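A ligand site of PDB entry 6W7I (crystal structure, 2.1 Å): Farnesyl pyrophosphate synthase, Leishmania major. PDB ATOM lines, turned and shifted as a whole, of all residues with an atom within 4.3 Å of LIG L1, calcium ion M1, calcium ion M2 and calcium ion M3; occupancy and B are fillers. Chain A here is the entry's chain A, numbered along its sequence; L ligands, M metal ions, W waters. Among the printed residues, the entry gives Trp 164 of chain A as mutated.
Of the 19 residues printed, 2 come within 4 Å of calcium ion M2.
The nearest printed residue that does not touch calcium ion M2 is Ser 104 (4.2 Å).
Water W5 bridges an oxygen (O6) of LIG L1 (2.6 Å) and the side-chain amide oxygen of Gln 167 (2.7 Å).
Water W1 lies within hydrogen-bond range of OD1 of Asp 170 (2.6 Å) and OD1 of Asp 102 (3.1 Å).
The side-chain amino group (NZ) of Lys 264 is in salt-bridge range of the side-chain carboxylate (OD1) of Asp 250 (2.7 Å).
The side-chain carboxylate (OD2) of Asp 250 sits close to the side-chain amide nitrogen (NE2) of Gln 247 (3.1 Å).
The side-chain carboxylate (OD1) of Asp 98 lies close to the side-chain amide nitrogen (NE2) of Gln 167 (3.0 Å).
The side-chain amino group (NZ) of Lys 207 lies within salt-bridge range of the side-chain carboxylate (OD2) of Asp 170 (2.9 Å).
OG1 of Thr 208 sits at hydrogen-bond distance from OE1 of Gln 247, 2.7 Å away.
SD of Met 101 lies close to NE2 of Gln 167 (3.6 Å).
Calcium ion M1 is bound by an oxygen (O1) of LIG L1 (2.2 Å), the side-chain carboxylate of Asp 250 (2.2 Å), an oxygen (O5) of LIG L1 (2.3 Å), water W3 (2.4 Å), water W7 (2.5 Å) and water W8 (2.5 Å).
Calcium ion M1 has six donor atoms within binding distance.
Two residues have an atom within 4 Å of calcium ion M3: Asp 98 and Asp 102.
The nearest printed residue that does not touch calcium ion M3 is Asp 170 (4.01 Å).
O6 of LIG L1 lies within salt-bridge range of NZ of Lys 207.
An oxygen (O2) of LIG L1 lies within salt-bridge range of the side-chain amino group (NZ) of Lys 264.
The guanidinium group (NH1) of Arg 107 is in salt-bridge range of an oxygen (O2) of LIG L1 (3.0 Å).
Calcium ion M3 is bound by OD2 of Asp 102 (2.3 Å), O4 of LIG L1 (2.4 Å), water W5 (2.4 Å), water W6 (2.4 Å), OD1 of Asp 98 (2.5 Å) and water W1 (2.5 Å).
Calcium ion M3 has six donor atoms within binding distance.
Slightly farther from calcium ion M3 lies OD1 of Asp 102 (3.0 Å).
Merely in contact with LIG L1: Phe 94 (3.5 Å), Met 101 (3.4 Å), Thr 163 (3.7 Å), Trp 164 (2.8 Å), Gln 167 (3.7 Å), Thr 208 (3.2 Å), Tyr 211 (3.8 Å) and Gln 247 (3.9 Å).
Within 4 Å of LIG L1: Phe 94, Asp 98, Met 101, Asp 102, Arg 107, Thr 163, Trp 164, Gln 167, Lys 207, Thr 208, Tyr 211, Gln 247, Asp 250 and Lys 264.
The nearest printed residue that does not touch LIG L1 is Leu 95 (4.2 Å).
Of the 19 residues printed, 1 comes within 4 Å of calcium ion M1.
The nearest printed residue that does not touch calcium ion M1 is Gln 247 (4.3 Å).
Water W9 binds calcium ion M2.
An oxygen (O3) of LIG L1 binds calcium ion M2 (2.2 Å).
OD2 of Asp 102 is bound to calcium ion M2 (2.3 Å).
OD2 of Asp 98 is bound to calcium ion M2, at 2.4 Å.
Calcium ion M2 is bound by water W2 (2.4 Å).
An oxygen (O4) of LIG L1 is bound to calcium ion M2 (2.5 Å).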
ATOM      1  N   PHE A  94     -17.663   9.863 -21.892  1.00  0.00           N
ATOM      2  CA  PHE A  94     -19.041   9.850 -21.334  1.00  0.00           C
ATOM      3  C   PHE A  94     -19.833  11.090 -21.742  1.00  0.00           C
ATOM      4  O   PHE A  94     -21.008  10.974 -22.073  1.00  0.00           O
ATOM      5  CB  PHE A  94     -19.042   9.759 -19.801  1.00  0.00           C
ATOM      6  CG  PHE A  94     -18.698   8.403 -19.255  1.00  0.00           C
ATOM      7  CD1 PHE A  94     -19.002   7.234 -19.957  1.00  0.00           C
ATOM      8  CD2 PHE A  94     -18.059   8.286 -18.028  1.00  0.00           C
ATOM      9  CE1 PHE A  94     -18.658   5.992 -19.443  1.00  0.00           C
ATOM     10  CE2 PHE A  94     -17.715   7.044 -17.494  1.00  0.00           C
ATOM     11  CZ  PHE A  94     -18.007   5.891 -18.206  1.00  0.00           C
ATOM     12  N   LEU A  95     -19.188  12.257 -21.692  1.00  0.00           N
ATOM     13  CA  LEU A  95     -19.886  13.521 -21.915  1.00  0.00           C
ATOM     14  C   LEU A  95     -20.147  13.784 -23.394  1.00  0.00           C
ATOM     15  O   LEU A  95     -21.211  14.275 -23.757  1.00  0.00           O
ATOM     16  CB  LEU A  95     -19.161  14.697 -21.230  1.00  0.00           C
ATOM     17  CG  LEU A  95     -18.797  14.568 -19.747  1.00  0.00           C
ATOM     18  CD1 LEU A  95     -18.227  15.891 -19.213  1.00  0.00           C
ATOM     19  CD2 LEU A  95     -20.001  14.114 -18.884  1.00  0.00           C
ATOM     20  N   GLU A  97     -20.708  11.423 -25.648  1.00  0.00           N
ATOM     21  CA  GLU A  97     -21.846  10.548 -25.927  1.00  0.00           C
ATOM     22  C   GLU A  97     -23.130  11.001 -25.239  1.00  0.00           C
ATOM     23  O   GLU A  97     -24.201  11.014 -25.857  1.00  0.00           O
ATOM     24  CB  GLU A  97     -21.531   9.093 -25.532  1.00  0.00           C
ATOM     25  CG  GLU A  97     -20.264   8.489 -26.179  1.00  0.00           C
ATOM     26  CD  GLU A  97     -20.272   8.487 -27.711  1.00  0.00           C
ATOM     27  OE1 GLU A  97     -21.301   8.833 -28.351  1.00  0.00           O
ATOM     28  OE2 GLU A  97     -19.227   8.111 -28.272  1.00  0.00           O
ATOM     29  N   ASP A  98     -23.034  11.395 -23.977  1.00  0.00           N
ATOM     30  CA  ASP A  98     -24.198  11.907 -23.264  1.00  0.00           C
ATOM     31  C   ASP A  98     -24.780  13.194 -23.872  1.00  0.00           C
ATOM     32  O   ASP A  98     -26.002  13.369 -23.918  1.00  0.00           O
ATOM     33  CB  ASP A  98     -23.905  12.133 -21.789  1.00  0.00           C
ATOM     34  CG  ASP A  98     -25.120  12.582 -21.028  1.00  0.00           C
ATOM     35  OD1 ASP A  98     -26.050  11.766 -20.906  1.00  0.00           O
ATOM     36  OD2 ASP A  98     -25.159  13.742 -20.584  1.00  0.00           O
ATOM     37  N   MET A 101     -26.853  12.134 -26.752  1.00  0.00           N
ATOM     38  CA  MET A 101     -28.033  11.406 -26.184  1.00  0.00           C
ATOM     39  C   MET A 101     -29.054  12.378 -25.579  1.00  0.00           C
ATOM     40  O   MET A 101     -30.183  12.330 -26.029  1.00  0.00           O
ATOM     41  CB  MET A 101     -27.612  10.392 -25.118  1.00  0.00           C
ATOM     42  CG  MET A 101     -27.002   9.129 -25.691  1.00  0.00           C
ATOM     43  SD  MET A 101     -26.610   7.857 -24.493  1.00  0.00           S
ATOM     44  CE  MET A 101     -25.266   8.621 -23.620  1.00  0.00           C
ATOM     45  N   ASP A 102     -28.561  13.443 -24.955  1.00  0.00           N
ATOM     46  CA  ASP A 102     -29.411  14.460 -24.332  1.00  0.00           C
ATOM     47  C   ASP A 102     -29.757  15.614 -25.276  1.00  0.00           C
ATOM     48  O   ASP A 102     -30.563  16.468 -24.938  1.00  0.00           O
ATOM     49  CB  ASP A 102     -28.735  15.005 -23.071  1.00  0.00           C
ATOM     50  CG  ASP A 102     -28.689  13.984 -21.944  1.00  0.00           C
ATOM     51  OD1 ASP A 102     -29.419  12.983 -22.021  1.00  0.00           O
ATOM     52  OD2 ASP A 102     -27.958  14.117 -20.936  1.00  0.00           O
ATOM     53  N   SER A 104     -27.946  18.143 -26.113  1.00  0.00           N
ATOM     54  CA  SER A 104     -27.604  19.305 -25.298  1.00  0.00           C
ATOM     55  C   SER A 104     -26.878  20.358 -26.124  1.00  0.00           C
ATOM     56  O   SER A 104     -26.484  20.104 -27.262  1.00  0.00           O
ATOM     57  CB  SER A 104     -26.754  18.866 -24.106  1.00  0.00           C
ATOM     58  OG  SER A 104     -27.527  18.108 -23.176  1.00  0.00           O
ATOM     59  N   ARG A 107     -21.198  22.583 -23.118  1.00  0.00           N
ATOM     60  CA  ARG A 107     -20.379  21.762 -22.254  1.00  0.00           C
ATOM     61  C   ARG A 107     -19.161  22.586 -21.859  1.00  0.00           C
ATOM     62  O   ARG A 107     -18.433  23.074 -22.738  1.00  0.00           O
ATOM     63  CB  ARG A 107     -19.942  20.459 -22.955  1.00  0.00           C
ATOM     64  CG  ARG A 107     -19.009  19.539 -22.114  1.00  0.00           C
ATOM     65  CD  ARG A 107     -19.643  19.130 -20.770  1.00  0.00           C
ATOM     66  NE  ARG A 107     -20.705  18.132 -20.934  1.00  0.00           N
ATOM     67  CZ  ARG A 107     -21.438  17.631 -19.935  1.00  0.00           C
ATOM     68  NH1 ARG A 107     -21.232  18.005 -18.667  1.00  0.00           N
ATOM     69  NH2 ARG A 107     -22.365  16.721 -20.193  1.00  0.00           N
ATOM     70  N   THR A 163     -21.190   2.306 -15.495  1.00  0.00           N
ATOM     71  CA  THR A 163     -21.654   3.648 -15.907  1.00  0.00           C
ATOM     72  C   THR A 163     -22.653   3.496 -17.059  1.00  0.00           C
ATOM     73  O   THR A 163     -23.654   4.153 -17.000  1.00  0.00           O
ATOM     74  CB  THR A 163     -20.484   4.601 -16.187  1.00  0.00           C
ATOM     75  OG1 THR A 163     -19.586   4.681 -15.089  1.00  0.00           O
ATOM     76  CG2 THR A 163     -20.976   5.976 -16.551  1.00  0.00           C
ATOM     77  N   TRP A 164     -22.355   2.618 -18.014  1.00  0.00           N
ATOM     78  CA  TRP A 164     -23.280   2.384 -19.151  1.00  0.00           C
ATOM     79  C   TRP A 164     -24.626   1.774 -18.724  1.00  0.00           C
ATOM     80  O   TRP A 164     -25.608   2.121 -19.321  1.00  0.00           O
ATOM     81  CB  TRP A 164     -22.587   1.728 -20.328  1.00  0.00           C
ATOM     82  CG  TRP A 164     -21.882   2.772 -21.125  1.00  0.00           C
ATOM     83  CD1 TRP A 164     -20.556   3.000 -21.239  1.00  0.00           C
ATOM     84  CD2 TRP A 164     -22.556   3.793 -21.855  1.00  0.00           C
ATOM     85  NE1 TRP A 164     -20.345   4.091 -22.022  1.00  0.00           N
ATOM     86  CE2 TRP A 164     -21.552   4.604 -22.423  1.00  0.00           C
ATOM     87  CE3 TRP A 164     -23.914   4.089 -22.100  1.00  0.00           C
ATOM     88  CZ2 TRP A 164     -21.882   5.693 -23.235  1.00  0.00           C
ATOM     89  CZ3 TRP A 164     -24.226   5.151 -22.901  1.00  0.00           C
ATOM     90  CH2 TRP A 164     -23.211   5.942 -23.478  1.00  0.00           C
ATOM     91  N   GLN A 167     -26.481   4.543 -17.124  1.00  0.00           N
ATOM     92  CA  GLN A 167     -26.999   5.343 -18.223  1.00  0.00           C
ATOM     93  C   GLN A 167     -28.273   4.744 -18.823  1.00  0.00           C
ATOM     94  O   GLN A 167     -29.190   5.475 -19.201  1.00  0.00           O
ATOM     95  CB  GLN A 167     -25.918   5.570 -19.290  1.00  0.00           C
ATOM     96  CG  GLN A 167     -26.351   6.494 -20.446  1.00  0.00           C
ATOM     97  CD  GLN A 167     -26.407   7.958 -20.067  1.00  0.00           C
ATOM     98  OE1 GLN A 167     -26.515   8.309 -18.885  1.00  0.00           O
ATOM     99  NE2 GLN A 167     -26.316   8.821 -21.074  1.00  0.00           N
ATOM    100  N   ASP A 170     -31.030   5.619 -16.576  1.00  0.00           N
ATOM    101  CA  ASP A 170     -31.328   7.030 -16.790  1.00  0.00           C
ATOM    102  C   ASP A 170     -32.194   7.295 -18.020  1.00  0.00           C
ATOM    103  O   ASP A 170     -33.193   8.024 -17.922  1.00  0.00           O
ATOM    104  CB  ASP A 170     -30.028   7.841 -16.851  1.00  0.00           C
ATOM    105  CG  ASP A 170     -30.269   9.310 -17.053  1.00  0.00           C
ATOM    106  OD1 ASP A 170     -30.683   9.718 -18.161  1.00  0.00           O
ATOM    107  OD2 ASP A 170     -30.052  10.073 -16.089  1.00  0.00           O
ATOM    108  N   LYS A 207     -24.554   5.380 -12.606  1.00  0.00           N
ATOM    109  CA  LYS A 207     -24.109   6.363 -13.616  1.00  0.00           C
ATOM    110  C   LYS A 207     -23.035   7.305 -13.101  1.00  0.00           C
ATOM    111  O   LYS A 207     -22.257   7.866 -13.888  1.00  0.00           O
ATOM    112  CB  LYS A 207     -25.291   7.139 -14.239  1.00  0.00           C
ATOM    113  CG  LYS A 207     -25.714   8.444 -13.527  1.00  0.00           C
ATOM    114  CD  LYS A 207     -26.618   9.317 -14.406  1.00  0.00           C
ATOM    115  CE  LYS A 207     -27.117  10.528 -13.617  1.00  0.00           C
ATOM    116  NZ  LYS A 207     -28.051  11.384 -14.428  1.00  0.00           N
ATOM    117  N   THR A 208     -22.959   7.512 -11.787  1.00  0.00           N
ATOM    118  CA  THR A 208     -22.047   8.539 -11.271  1.00  0.00           C
ATOM    119  C   THR A 208     -21.032   8.091 -10.211  1.00  0.00           C
ATOM    120  O   THR A 208     -19.835   8.330 -10.361  1.00  0.00           O
ATOM    121  CB  THR A 208     -22.830   9.797 -10.807  1.00  0.00           C
ATOM    122  OG1 THR A 208     -23.488  10.378 -11.941  1.00  0.00           O
ATOM    123  CG2 THR A 208     -21.899  10.857 -10.181  1.00  0.00           C
ATOM    124  N   TYR A 211     -17.668   5.804 -11.166  1.00  0.00           N
ATOM    125  CA  TYR A 211     -16.594   6.442 -11.949  1.00  0.00           C
ATOM    126  C   TYR A 211     -16.044   7.742 -11.365  1.00  0.00           C
ATOM    127  O   TYR A 211     -14.886   8.087 -11.609  1.00  0.00           O
ATOM    128  CB  TYR A 211     -16.975   6.596 -13.433  1.00  0.00           C
ATOM    129  CG  TYR A 211     -17.604   7.915 -13.903  1.00  0.00           C
ATOM    130  CD1 TYR A 211     -18.988   8.134 -13.829  1.00  0.00           C
ATOM    131  CD2 TYR A 211     -16.815   8.903 -14.505  1.00  0.00           C
ATOM    132  CE1 TYR A 211     -19.571   9.330 -14.305  1.00  0.00           C
ATOM    133  CE2 TYR A 211     -17.383  10.087 -14.970  1.00  0.00           C
ATOM    134  CZ  TYR A 211     -18.760  10.300 -14.875  1.00  0.00           C
ATOM    135  OH  TYR A 211     -19.299  11.488 -15.359  1.00  0.00           O
ATOM    136  N   GLN A 247     -24.199  13.640  -7.332  1.00  0.00           N
ATOM    137  CA  GLN A 247     -25.229  13.672  -8.388  1.00  0.00           C
ATOM    138  C   GLN A 247     -26.488  14.415  -7.973  1.00  0.00           C
ATOM    139  O   GLN A 247     -27.122  15.069  -8.796  1.00  0.00           O
ATOM    140  CB  GLN A 247     -25.589  12.264  -8.891  1.00  0.00           C
ATOM    141  CG  GLN A 247     -26.419  12.239 -10.196  1.00  0.00           C
ATOM    142  CD  GLN A 247     -25.768  13.020 -11.333  1.00  0.00           C
ATOM    143  OE1 GLN A 247     -24.597  12.831 -11.639  1.00  0.00           O
ATOM    144  NE2 GLN A 247     -26.556  13.899 -11.976  1.00  0.00           N
ATOM    145  N   ASP A 250     -25.665  17.890  -8.664  1.00  0.00           N
ATOM    146  CA  ASP A 250     -25.800  18.107 -10.106  1.00  0.00           C
ATOM    147  C   ASP A 250     -27.260  18.272 -10.506  1.00  0.00           C
ATOM    148  O   ASP A 250     -27.584  19.154 -11.295  1.00  0.00           O
ATOM    149  CB  ASP A 250     -25.167  16.958 -10.880  1.00  0.00           C
ATOM    150  CG  ASP A 250     -25.019  17.263 -12.358  1.00  0.00           C
ATOM    151  OD1 ASP A 250     -24.198  18.132 -12.716  1.00  0.00           O
ATOM    152  OD2 ASP A 250     -25.717  16.609 -13.168  1.00  0.00           O
ATOM    153  N   LYS A 264     -23.075  24.599 -18.636  1.00  0.00           N
ATOM    154  CA  LYS A 264     -23.909  23.658 -19.369  1.00  0.00           C
ATOM    155  C   LYS A 264     -25.376  24.011 -19.170  1.00  0.00           C
ATOM    156  O   LYS A 264     -25.734  24.632 -18.155  1.00  0.00           O
ATOM    157  CB  LYS A 264     -23.618  22.207 -18.925  1.00  0.00           C
ATOM    158  CG  LYS A 264     -23.890  21.921 -17.454  1.00  0.00           C
ATOM    159  CD  LYS A 264     -23.252  20.632 -16.963  1.00  0.00           C
ATOM    160  CE  LYS A 264     -23.744  20.301 -15.543  1.00  0.00           C
ATOM    161  NZ  LYS A 264     -23.256  18.963 -15.060  1.00  0.00           N
ATOM    162  N   ASP A 268     -33.332  18.544 -17.730  1.00  0.00           N
ATOM    163  CA  ASP A 268     -33.982  17.508 -16.900  1.00  0.00           C
ATOM    164  C   ASP A 268     -35.493  17.724 -16.862  1.00  0.00           C
ATOM    165  O   ASP A 268     -36.209  16.762 -16.918  1.00  0.00           O
ATOM    166  CB  ASP A 268     -33.345  17.451 -15.503  1.00  0.00           C
ATOM    167  CG  ASP A 268     -31.967  16.805 -15.433  1.00  0.00           C
ATOM    168  OD1 ASP A 268     -31.426  16.423 -16.471  1.00  0.00           O
ATOM    169  OD2 ASP A 268     -31.444  16.755 -14.343  1.00  0.00           O
HETATM  170  O1  LIG L   1     -25.625  17.217 -16.315  1.00  0.00           O
HETATM  171  P1  LIG L   1     -24.657  16.468 -17.176  1.00  0.00           P
HETATM  172  O2  LIG L   1     -23.230  16.783 -16.854  1.00  0.00           O
HETATM  173  O3  LIG L   1     -24.923  16.510 -18.653  1.00  0.00           O
HETATM  174  C1  LIG L   1     -24.842  14.712 -16.653  1.00  0.00           C
HETATM  175  P2  LIG L   1     -26.550  14.073 -16.625  1.00  0.00           P
HETATM  176  O4  LIG L   1     -27.037  14.092 -18.053  1.00  0.00           O
HETATM  177  O5  LIG L   1     -27.333  14.941 -15.666  1.00  0.00           O
HETATM  178  O6  LIG L   1     -26.462  12.661 -16.082  1.00  0.00           O
HETATM  179  C2  LIG L   1     -23.992  13.803 -17.558  1.00  0.00           C
HETATM  180  N1  LIG L   1     -23.653  12.512 -16.954  1.00  0.00           N
HETATM  181  C3  LIG L   1     -23.407  11.431 -17.748  1.00  0.00           C
HETATM  182  C4  LIG L   1     -23.060  10.198 -17.174  1.00  0.00           C
HETATM  183  C5  LIG L   1     -22.975  10.058 -15.796  1.00  0.00           C
HETATM  184  C6  LIG L   1     -23.217  11.161 -15.001  1.00  0.00           C
HETATM  185  C7  LIG L   1     -23.560  12.380 -15.615  1.00  0.00           C
HETATM  186  C8  LIG L   1     -22.783   8.942 -17.965  1.00  0.00           C
HETATM  187  C9  LIG L   1     -22.744   9.118 -19.467  1.00  0.00           C
HETATM  188  C10 LIG L   1     -22.721   7.724 -20.100  1.00  0.00           C
HETATM  189  C11 LIG L   1     -22.667   7.938 -21.592  1.00  0.00           C
HETATM  190  P1  LG2 L   2     -16.268  18.213 -15.263  1.00  0.00           P
HETATM  191  O1  LG2 L   2     -15.565  16.965 -15.731  1.00  0.00           O
HETATM  192  O2  LG2 L   2     -16.572  19.177 -16.382  1.00  0.00           O
HETATM  193  O3  LG2 L   2     -15.681  18.775 -13.987  1.00  0.00           O
HETATM  194  O4  LG2 L   2     -17.782  17.757 -14.896  1.00  0.00           O
HETATM  195  P2  LG2 L   2     -18.327  17.016 -13.564  1.00  0.00           P
HETATM  196  O5  LG2 L   2     -17.192  16.423 -12.776  1.00  0.00           O
HETATM  197  O6  LG2 L   2     -19.253  17.975 -12.853  1.00  0.00           O
HETATM  198  O7  LG2 L   2     -19.209  15.793 -14.146  1.00  0.00           O
HETATM  199  C1  LG2 L   2     -20.255  15.973 -15.125  1.00  0.00           C
HETATM  200  C2  LG2 L   2     -21.173  14.749 -15.128  1.00  0.00           C
HETATM  201  C3  LG2 L   2     -21.622  14.373 -13.735  1.00  0.00           C
HETATM  202  C4  LG2 L   2     -21.090  13.123 -13.090  1.00  0.00           C
HETATM  203  C5  LG2 L   2     -22.475  15.126 -13.048  1.00  0.00           C
HETATM  204 CA    CA M   1     -27.207  17.031 -14.794  1.00  0.00          CA
HETATM  205 CA    CA M   2     -26.481  15.580 -19.925  1.00  0.00          CA
HETATM  206 CA    CA M   3     -27.974  12.381 -19.453  1.00  0.00          CA
HETATM  207  O   HOH W   1     -29.335  10.410 -20.262  1.00  0.00           O
HETATM  208  O   HOH W   2     -28.106  17.302 -19.471  1.00  0.00           O
HETATM  209  O   HOH W   3     -29.041  16.374 -13.350  1.00  0.00           O
HETATM  210  O   HOH W   4     -30.118  14.186 -15.903  1.00  0.00           O
HETATM  211  O   HOH W   5     -26.920  10.849 -17.917  1.00  0.00           O
HETATM  212  O   HOH W   6     -29.825  12.574 -17.871  1.00  0.00           O
HETATM  213  O   HOH W   7     -26.928  19.374 -14.097  1.00  0.00           O
HETATM  214  O   HOH W   8     -29.095  17.824 -16.185  1.00  0.00           O
HETATM  215  O   HOH W   9     -25.841  16.602 -21.777  1.00  0.00           O
